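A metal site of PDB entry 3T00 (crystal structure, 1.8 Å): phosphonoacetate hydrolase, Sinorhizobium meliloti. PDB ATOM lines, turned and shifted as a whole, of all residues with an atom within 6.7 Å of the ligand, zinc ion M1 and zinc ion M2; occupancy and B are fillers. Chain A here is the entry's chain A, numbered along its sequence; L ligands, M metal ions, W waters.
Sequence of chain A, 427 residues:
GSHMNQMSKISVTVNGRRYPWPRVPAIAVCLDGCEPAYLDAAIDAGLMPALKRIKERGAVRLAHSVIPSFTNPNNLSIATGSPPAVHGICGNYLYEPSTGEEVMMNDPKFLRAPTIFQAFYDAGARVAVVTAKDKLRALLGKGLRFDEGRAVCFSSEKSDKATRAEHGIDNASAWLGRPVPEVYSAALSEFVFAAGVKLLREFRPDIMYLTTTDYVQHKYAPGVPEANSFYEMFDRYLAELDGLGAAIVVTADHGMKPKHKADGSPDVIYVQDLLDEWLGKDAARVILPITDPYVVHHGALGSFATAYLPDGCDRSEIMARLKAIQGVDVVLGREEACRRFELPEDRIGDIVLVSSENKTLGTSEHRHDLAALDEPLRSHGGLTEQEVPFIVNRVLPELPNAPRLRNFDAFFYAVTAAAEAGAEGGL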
ATOM      1  N   CYS A  30       2.694  -8.311  24.372  1.00  0.00           N
ATOM      2  CA  CYS A  30       3.053  -8.948  23.104  1.00  0.00           C
ATOM      3  C   CYS A  30       2.830  -7.963  21.975  1.00  0.00           C
ATOM      4  O   CYS A  30       1.678  -7.689  21.612  1.00  0.00           O
ATOM      5  CB  CYS A  30       2.226 -10.205  22.862  1.00  0.00           C
ATOM      6  SG  CYS A  30       2.591 -11.056  21.293  1.00  0.00           S
ATOM      7  N   ASP A  32       2.707  -7.701  18.493  1.00  0.00           N
ATOM      8  CA  ASP A  32       2.531  -8.628  17.376  1.00  0.00           C
ATOM      9  C   ASP A  32       3.390  -8.231  16.180  1.00  0.00           C
ATOM     10  O   ASP A  32       3.364  -7.085  15.724  1.00  0.00           O
ATOM     11  CB  ASP A  32       1.050  -8.634  16.977  1.00  0.00           C
ATOM     12  CG  ASP A  32       0.647  -9.901  16.282  1.00  0.00           C
ATOM     13  OD1 ASP A  32       1.347 -10.306  15.329  1.00  0.00           O
ATOM     14  OD2 ASP A  32      -0.379 -10.499  16.695  1.00  0.00           O
ATOM     15  N   GLY A  33       4.184  -9.180  15.681  1.00  0.00           N
ATOM     16  CA  GLY A  33       4.992  -8.972  14.479  1.00  0.00           C
ATOM     17  C   GLY A  33       6.140  -7.978  14.634  1.00  0.00           C
ATOM     18  O   GLY A  33       6.688  -7.495  13.646  1.00  0.00           O
ATOM     19  N   SER A  69       6.521 -19.549  13.422  1.00  0.00           N
ATOM     20  CA  SER A  69       6.457 -18.192  13.966  1.00  0.00           C
ATOM     21  C   SER A  69       5.154 -17.509  13.516  1.00  0.00           C
ATOM     22  O   SER A  69       5.164 -16.536  12.755  1.00  0.00           O
ATOM     23  CB  SER A  69       7.721 -17.389  13.598  1.00  0.00           C
ATOM     24  OG  SER A  69       7.968 -17.364  12.196  1.00  0.00           O
ATOM     25  N   PHE A  70       4.030 -18.049  14.002  1.00  0.00           N
ATOM     26  CA  PHE A  70       2.692 -17.490  13.755  1.00  0.00           C
ATOM     27  C   PHE A  70       2.057 -17.019  15.070  1.00  0.00           C
ATOM     28  O   PHE A  70       2.536 -17.353  16.147  1.00  0.00           O
ATOM     29  CB  PHE A  70       1.763 -18.537  13.105  1.00  0.00           C
ATOM     30  CG  PHE A  70       2.160 -18.945  11.705  1.00  0.00           C
ATOM     31  CD1 PHE A  70       2.549 -17.997  10.761  1.00  0.00           C
ATOM     32  CD2 PHE A  70       2.108 -20.280  11.318  1.00  0.00           C
ATOM     33  CE1 PHE A  70       2.912 -18.366   9.461  1.00  0.00           C
ATOM     34  CE2 PHE A  70       2.457 -20.666  10.015  1.00  0.00           C
ATOM     35  CZ  PHE A  70       2.871 -19.714   9.092  1.00  0.00           C
ATOM     36  N   THR A  71       0.968 -16.273  14.961  1.00  0.00           N
ATOM     37  CA  THR A  71       0.311 -15.610  16.095  1.00  0.00           C
ATOM     38  C   THR A  71      -0.223 -16.540  17.166  1.00  0.00           C
ATOM     39  O   THR A  71       0.169 -16.454  18.324  1.00  0.00           O
ATOM     40  CB  THR A  71      -0.878 -14.741  15.612  1.00  0.00           C
ATOM     41  OG1 THR A  71      -0.405 -13.853  14.601  1.00  0.00           O
ATOM     42  CG2 THR A  71      -1.485 -13.926  16.753  1.00  0.00           C
ATOM     43  N   ASN A  72      -1.146 -17.426  16.782  1.00  0.00           N
ATOM     44  CA  ASN A  72      -1.776 -18.317  17.740  1.00  0.00           C
ATOM     45  C   ASN A  72      -0.822 -19.255  18.479  1.00  0.00           C
ATOM     46  O   ASN A  72      -0.872 -19.309  19.710  1.00  0.00           O
ATOM     47  CB  ASN A  72      -2.980 -19.047  17.124  1.00  0.00           C
ATOM     48  CG  ASN A  72      -4.194 -18.142  16.998  1.00  0.00           C
ATOM     49  OD1 ASN A  72      -4.084 -16.923  17.157  1.00  0.00           O
ATOM     50  ND2 ASN A  72      -5.349 -18.737  16.738  1.00  0.00           N
ATOM     51  N   PRO A  73       0.073 -19.981  17.756  1.00  0.00           N
ATOM     52  CA  PRO A  73       0.979 -20.871  18.513  1.00  0.00           C
ATOM     53  C   PRO A  73       1.838 -20.105  19.506  1.00  0.00           C
ATOM     54  O   PRO A  73       2.058 -20.566  20.632  1.00  0.00           O
ATOM     55  CB  PRO A  73       1.848 -21.506  17.429  1.00  0.00           C
ATOM     56  CG  PRO A  73       1.051 -21.356  16.166  1.00  0.00           C
ATOM     57  CD  PRO A  73       0.268 -20.099  16.293  1.00  0.00           C
ATOM     58  N   ASN A  75       1.249 -16.860  20.876  1.00  0.00           N
ATOM     59  CA  ASN A  75       0.434 -16.287  21.950  1.00  0.00           C
ATOM     60  C   ASN A  75       0.051 -17.347  22.982  1.00  0.00           C
ATOM     61  O   ASN A  75       0.102 -17.108  24.183  1.00  0.00           O
ATOM     62  CB  ASN A  75      -0.806 -15.581  21.384  1.00  0.00           C
ATOM     63  CG  ASN A  75      -0.515 -14.152  20.991  1.00  0.00           C
ATOM     64  OD1 ASN A  75      -0.144 -13.873  19.845  1.00  0.00           O
ATOM     65  ND2 ASN A  75      -0.670 -13.240  21.936  1.00  0.00           N
ATOM     66  N   ASN A  92      -3.700 -22.534  12.827  1.00  0.00           N
ATOM     67  CA  ASN A  92      -5.052 -21.964  12.880  1.00  0.00           C
ATOM     68  C   ASN A  92      -6.148 -22.969  12.551  1.00  0.00           C
ATOM     69  O   ASN A  92      -7.323 -22.731  12.841  1.00  0.00           O
ATOM     70  CB  ASN A  92      -5.157 -20.731  11.976  1.00  0.00           C
ATOM     71  CG  ASN A  92      -4.635 -19.470  12.653  1.00  0.00           C
ATOM     72  OD1 ASN A  92      -4.219 -19.496  13.814  1.00  0.00           O
ATOM     73  ND2 ASN A  92      -4.667 -18.363  11.929  1.00  0.00           N
ATOM     74  N   LYS A 135     -11.185 -13.913  18.834  1.00  0.00           N
ATOM     75  CA  LYS A 135     -11.028 -15.382  18.851  1.00  0.00           C
ATOM     76  C   LYS A 135      -9.838 -15.795  19.724  1.00  0.00           C
ATOM     77  O   LYS A 135      -9.901 -16.811  20.432  1.00  0.00           O
ATOM     78  CB  LYS A 135     -11.022 -16.010  17.441  1.00  0.00           C
ATOM     79  CG  LYS A 135      -9.817 -15.761  16.558  1.00  0.00           C
ATOM     80  CD  LYS A 135      -8.804 -16.908  16.634  1.00  0.00           C
ATOM     81  CE  LYS A 135      -8.147 -17.194  15.293  1.00  0.00           C
ATOM     82  NZ  LYS A 135      -7.308 -16.079  14.794  1.00  0.00           N
ATOM     83  N   THR A 212      -1.627  -7.719  20.810  1.00  0.00           N
ATOM     84  CA  THR A 212      -2.049  -6.794  19.757  1.00  0.00           C
ATOM     85  C   THR A 212      -2.215  -7.536  18.423  1.00  0.00           C
ATOM     86  O   THR A 212      -2.332  -8.764  18.421  1.00  0.00           O
ATOM     87  CB  THR A 212      -1.048  -5.633  19.633  1.00  0.00           C
ATOM     88  OG1 THR A 212       0.269  -6.150  19.398  1.00  0.00           O
ATOM     89  CG2 THR A 212      -1.020  -4.820  20.915  1.00  0.00           C
ATOM     90  N   THR A 213      -2.254  -6.798  17.298  1.00  0.00           N
ATOM     91  CA  THR A 213      -2.194  -7.405  15.951  1.00  0.00           C
ATOM     92  C   THR A 213      -1.057  -6.819  15.120  1.00  0.00           C
ATOM     93  O   THR A 213      -0.568  -5.733  15.424  1.00  0.00           O
ATOM     94  CB  THR A 213      -3.508  -7.268  15.117  1.00  0.00           C
ATOM     95  OG1 THR A 213      -3.597  -5.941  14.563  1.00  0.00           O
ATOM     96  CG2 THR A 213      -4.738  -7.562  15.958  1.00  0.00           C
ATOM     97  N   ASP A 214      -0.655  -7.538  14.075  1.00  0.00           N
ATOM     98  CA  ASP A 214       0.460  -7.105  13.215  1.00  0.00           C
ATOM     99  C   ASP A 214      -0.016  -6.443  11.898  1.00  0.00           C
ATOM    100  O   ASP A 214       0.685  -6.478  10.880  1.00  0.00           O
ATOM    101  CB  ASP A 214       1.452  -8.253  12.952  1.00  0.00           C
ATOM    102  CG  ASP A 214       0.823  -9.421  12.198  1.00  0.00           C
ATOM    103  OD1 ASP A 214      -0.406  -9.457  11.986  1.00  0.00           O
ATOM    104  OD2 ASP A 214       1.594 -10.337  11.806  1.00  0.00           O
ATOM    105  N   TYR A 215      -1.191  -5.834  11.961  1.00  0.00           N
ATOM    106  CA  TYR A 215      -1.732  -5.064  10.833  1.00  0.00           C
ATOM    107  C   TYR A 215      -0.712  -4.071  10.259  1.00  0.00           C
ATOM    108  O   TYR A 215      -0.414  -4.104   9.054  1.00  0.00           O
ATOM    109  CB  TYR A 215      -3.028  -4.342  11.227  1.00  0.00           C
ATOM    110  CG  TYR A 215      -3.478  -3.384  10.142  1.00  0.00           C
ATOM    111  CD1 TYR A 215      -4.072  -3.858   8.973  1.00  0.00           C
ATOM    112  CD2 TYR A 215      -3.247  -2.012  10.254  1.00  0.00           C
ATOM    113  CE1 TYR A 215      -4.453  -2.999   7.947  1.00  0.00           C
ATOM    114  CE2 TYR A 215      -3.626  -1.138   9.239  1.00  0.00           C
ATOM    115  CZ  TYR A 215      -4.227  -1.636   8.096  1.00  0.00           C
ATOM    116  OH  TYR A 215      -4.608  -0.770   7.092  1.00  0.00           O
ATOM    117  N   HIS A 218       2.614  -5.862   8.784  1.00  0.00           N
ATOM    118  CA  HIS A 218       2.445  -6.519   7.482  1.00  0.00           C
ATOM    119  C   HIS A 218       2.489  -5.500   6.335  1.00  0.00           C
ATOM    120  O   HIS A 218       2.870  -5.831   5.201  1.00  0.00           O
ATOM    121  CB  HIS A 218       1.130  -7.282   7.425  1.00  0.00           C
ATOM    122  CG  HIS A 218       1.221  -8.699   7.926  1.00  0.00           C
ATOM    123  ND1 HIS A 218       1.879  -9.692   7.236  1.00  0.00           N
ATOM    124  CD2 HIS A 218       0.725  -9.272   9.047  1.00  0.00           C
ATOM    125  CE1 HIS A 218       1.778 -10.828   7.910  1.00  0.00           C
ATOM    126  NE2 HIS A 218       1.098 -10.599   9.011  1.00  0.00           N
ATOM    127  N   ASP A 253       5.204 -12.095  19.493  1.00  0.00           N
ATOM    128  CA  ASP A 253       4.894 -13.466  19.055  1.00  0.00           C
ATOM    129  C   ASP A 253       5.810 -13.991  17.947  1.00  0.00           C
ATOM    130  O   ASP A 253       6.088 -15.188  17.861  1.00  0.00           O
ATOM    131  CB  ASP A 253       3.417 -13.608  18.658  1.00  0.00           C
ATOM    132  CG  ASP A 253       2.971 -12.580  17.613  1.00  0.00           C
ATOM    133  OD1 ASP A 253       3.743 -11.655  17.234  1.00  0.00           O
ATOM    134  OD2 ASP A 253       1.806 -12.702  17.202  1.00  0.00           O
ATOM    135  N   HIS A 254       6.267 -13.070  17.094  1.00  0.00           N
ATOM    136  CA  HIS A 254       7.135 -13.379  15.958  1.00  0.00           C
ATOM    137  C   HIS A 254       7.594 -12.060  15.343  1.00  0.00           C
ATOM    138  O   HIS A 254       7.058 -11.014  15.686  1.00  0.00           O
ATOM    139  CB  HIS A 254       6.380 -14.181  14.900  1.00  0.00           C
ATOM    140  CG  HIS A 254       5.093 -13.540  14.465  1.00  0.00           C
ATOM    141  ND1 HIS A 254       5.051 -12.470  13.594  1.00  0.00           N
ATOM    142  CD2 HIS A 254       3.812 -13.805  14.805  1.00  0.00           C
ATOM    143  CE1 HIS A 254       3.799 -12.102  13.424  1.00  0.00           C
ATOM    144  NE2 HIS A 254       3.031 -12.891  14.145  1.00  0.00           N
ATOM    145  N   GLY A 255       8.559 -12.141  14.442  1.00  0.00           N
ATOM    146  CA  GLY A 255       9.063 -10.981  13.715  1.00  0.00           C
ATOM    147  C   GLY A 255       8.334 -10.781  12.400  1.00  0.00           C
ATOM    148  O   GLY A 255       7.185 -11.206  12.230  1.00  0.00           O
ATOM    149  N   MET A 256       9.020 -10.139  11.456  1.00  0.00           N
ATOM    150  CA  MET A 256       8.409  -9.769  10.184  1.00  0.00           C
ATOM    151  C   MET A 256       9.521  -9.495   9.188  1.00  0.00           C
ATOM    152  O   MET A 256      10.473  -8.795   9.500  1.00  0.00           O
ATOM    153  CB  MET A 256       7.526  -8.518  10.365  1.00  0.00           C
ATOM    154  CG  MET A 256       6.627  -8.174   9.173  1.00  0.00           C
ATOM    155  SD  MET A 256       5.277  -9.341   8.871  1.00  0.00           S
ATOM    156  CE  MET A 256       4.153  -8.972  10.202  1.00  0.00           C
ATOM    157  N   PRO A 289      -0.746 -23.153   7.909  1.00  0.00           N
ATOM    158  CA  PRO A 289      -1.256 -22.840   9.241  1.00  0.00           C
ATOM    159  C   PRO A 289      -1.410 -21.345   9.570  1.00  0.00           C
ATOM    160  O   PRO A 289      -2.027 -21.022  10.587  1.00  0.00           O
ATOM    161  CB  PRO A 289      -0.218 -23.478  10.185  1.00  0.00           C
ATOM    162  CG  PRO A 289       0.559 -24.427   9.322  1.00  0.00           C
ATOM    163  CD  PRO A 289       0.586 -23.797   7.976  1.00  0.00           C
ATOM    164  N   ILE A 290      -0.871 -20.461   8.726  1.00  0.00           N
ATOM    165  CA  ILE A 290      -0.860 -19.013   8.997  1.00  0.00           C
ATOM    166  C   ILE A 290      -2.245 -18.426   9.324  1.00  0.00           C
ATOM    167  O   ILE A 290      -2.385 -17.663  10.288  1.00  0.00           O
ATOM    168  CB  ILE A 290      -0.165 -18.188   7.870  1.00  0.00           C
ATOM    169  CG1 ILE A 290      -0.119 -16.695   8.244  1.00  0.00           C
ATOM    170  CG2 ILE A 290      -0.831 -18.406   6.508  1.00  0.00           C
ATOM    171  CD1 ILE A 290       0.921 -15.878   7.493  1.00  0.00           C
ATOM    172  N   THR A 291      -3.245 -18.788   8.533  1.00  0.00           N
ATOM    173  CA  THR A 291      -4.614 -18.293   8.747  1.00  0.00           C
ATOM    174  C   THR A 291      -5.672 -19.213   8.128  1.00  0.00           C
ATOM    175  O   THR A 291      -5.343 -20.140   7.381  1.00  0.00           O
ATOM    176  CB  THR A 291      -4.790 -16.828   8.271  1.00  0.00           C
ATOM    177  OG1 THR A 291      -6.078 -16.342   8.668  1.00  0.00           O
ATOM    178  CG2 THR A 291      -4.635 -16.705   6.753  1.00  0.00           C
ATOM    179  N   GLY A 299      -3.680 -13.152   2.043  1.00  0.00           N
ATOM    180  CA  GLY A 299      -3.426 -13.177   3.480  1.00  0.00           C
ATOM    181  C   GLY A 299      -2.977 -14.518   4.011  1.00  0.00           C
ATOM    182  O   GLY A 299      -2.615 -14.639   5.187  1.00  0.00           O
ATOM    183  N   ARG A 378       4.856  -8.602   3.044  1.00  0.00           N
ATOM    184  CA  ARG A 378       5.644  -8.809   4.258  1.00  0.00           C
ATOM    185  C   ARG A 378       4.938  -9.893   5.059  1.00  0.00           C
ATOM    186  O   ARG A 378       3.713  -9.859   5.213  1.00  0.00           O
ATOM    187  CB  ARG A 378       5.734  -7.524   5.087  1.00  0.00           C
ATOM    188  CG  ARG A 378       6.415  -6.362   4.371  1.00  0.00           C
ATOM    189  CD  ARG A 378       6.389  -5.077   5.205  1.00  0.00           C
ATOM    190  NE  ARG A 378       6.975  -5.268   6.538  1.00  0.00           N
ATOM    191  CZ  ARG A 378       8.273  -5.401   6.779  1.00  0.00           C
ATOM    192  NH1 ARG A 378       9.157  -5.384   5.790  1.00  0.00           N
ATOM    193  NH2 ARG A 378       8.689  -5.582   8.032  1.00  0.00           N
ATOM    194  N   SER A 379       5.700 -10.853   5.564  1.00  0.00           N
ATOM    195  CA  SER A 379       5.090 -11.933   6.335  1.00  0.00           C
ATOM    196  C   SER A 379       6.064 -12.584   7.306  1.00  0.00           C
ATOM    197  O   SER A 379       7.164 -12.070   7.549  1.00  0.00           O
ATOM    198  CB  SER A 379       4.446 -12.981   5.421  1.00  0.00           C
ATOM    199  OG  SER A 379       3.402 -13.645   6.105  1.00  0.00           O
ATOM    200  N   HIS A 380       5.637 -13.720   7.826  1.00  0.00           N
ATOM    201  CA  HIS A 380       6.367 -14.439   8.872  1.00  0.00           C
ATOM    202  C   HIS A 380       6.015 -15.917   8.846  1.00  0.00           C
ATOM    203  O   HIS A 380       5.323 -16.404   7.916  1.00  0.00           O
ATOM    204  CB  HIS A 380       6.054 -13.813  10.240  1.00  0.00           C
ATOM    205  CG  HIS A 380       4.597 -13.608  10.479  1.00  0.00           C
ATOM    206  ND1 HIS A 380       3.794 -14.536  11.110  1.00  0.00           N
ATOM    207  CD2 HIS A 380       3.774 -12.573  10.139  1.00  0.00           C
ATOM    208  CE1 HIS A 380       2.559 -14.089  11.159  1.00  0.00           C
ATOM    209  NE2 HIS A 380       2.520 -12.896  10.587  1.00  0.00           N
HETATM  210  V1  LIG L   1      -0.681 -13.540  12.610  1.00  0.00           V
HETATM  211  O1  LIG L   1      -2.431 -13.359  13.301  1.00  0.00           O
HETATM  212  O2  LIG L   1      -0.707 -12.848  10.828  1.00  0.00           O
HETATM  213  O3  LIG L   1      -0.129 -15.378  12.501  1.00  0.00           O
HETATM  214  O4  LIG L   1       0.641 -12.385  13.349  1.00  0.00           O
HETATM  215 ZN    ZN M   1       0.871 -11.683  10.826  1.00  0.00          ZN
HETATM  216 ZN    ZN M   2       1.151 -12.277  15.076  1.00  0.00          ZN
HETATM  217  O   HOH W   1      -1.970 -10.606  14.572  1.00  0.00           O
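Zinc ion M2 is bound by O4 of the ligand, OD1 of Asp 32, NE2 of His 254, OD2 of Asp 253 and OG1 of Thr 71. Zinc ion M2 has five donor atoms within binding distance.
A vanadium atom (V1) of the ligand is bound by the side-chain hydroxyl (OG1) of Thr 71.
Water W1 bridges OD2 of Asp 32 and OD1 of Asp 214.
Of the 27 residues printed, 4 come within 4 Å of zinc ion M1. The nearest printed residue that does not touch zinc ion M1 is Met 256 (4.3 Å).
SG of Cys 30 sits at hydrogen-bond distance from N of Asp 253 (3.3 Å). The backbone NH of Asp 32 sits at hydrogen-bond distance from the side-chain hydroxyl of Thr 212, 3.0 Å away. The side-chain amide oxygen (OD1) of Asn 75 sits close to the backbone carbonyl oxygen (O) of Thr 71. The side-chain carboxylate (OD2) of Asp 253 sits close to the side-chain amide oxygen (OD1) of Asn 75, at 3.5 Å. The backbone carbonyl oxygen (O) of His 254 lies close to the backbone NH (N) of Gly 33. A ring nitrogen (ND1) of His 218 is in hydrogen-bond range of the backbone carbonyl oxygen of Arg 378 (2.7 Å). A ring nitrogen (ND1) of His 380 lies close to a ring nitrogen (ND1) of His 254 (3.5 Å). The backbone NH (N) of Gly 33 lies within hydrogen-bond range of the side-chain carboxylate (OD1) of Asp 253 (3.0 Å).
Phe 70 touches the ligand (CB to O3, 3.7 Å). O of Ile 290 touches O3 of the ligand, at 3.9 Å. Hydrophobic or aromatic side chains within 4 Å of the ligand: Phe 70, His 254 and His 380. Of the 27 residues printed, 8 come within 4 Å of the ligand.
Zinc ion M1 is bound by OD2 of Asp 214 (1.8 Å), O2 of the ligand (2.0 Å), NE2 of His 380 (2.1 Å) and NE2 of His 218 (2.1 Å). Zinc ion M1 has four donor atoms within binding distance. Slightly farther from zinc ion M1 lies O4 of the ligand (2.6 Å). Slightly farther from zinc ion M1 lies the side-chain carboxylate (OD1) of Asp 214 (2.8 Å).
Of the 27 residues printed, 5 come within 4 Å of zinc ion M2. The nearest printed residue that does not touch zinc ion M2 is Gly 33 (4.4 Å).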
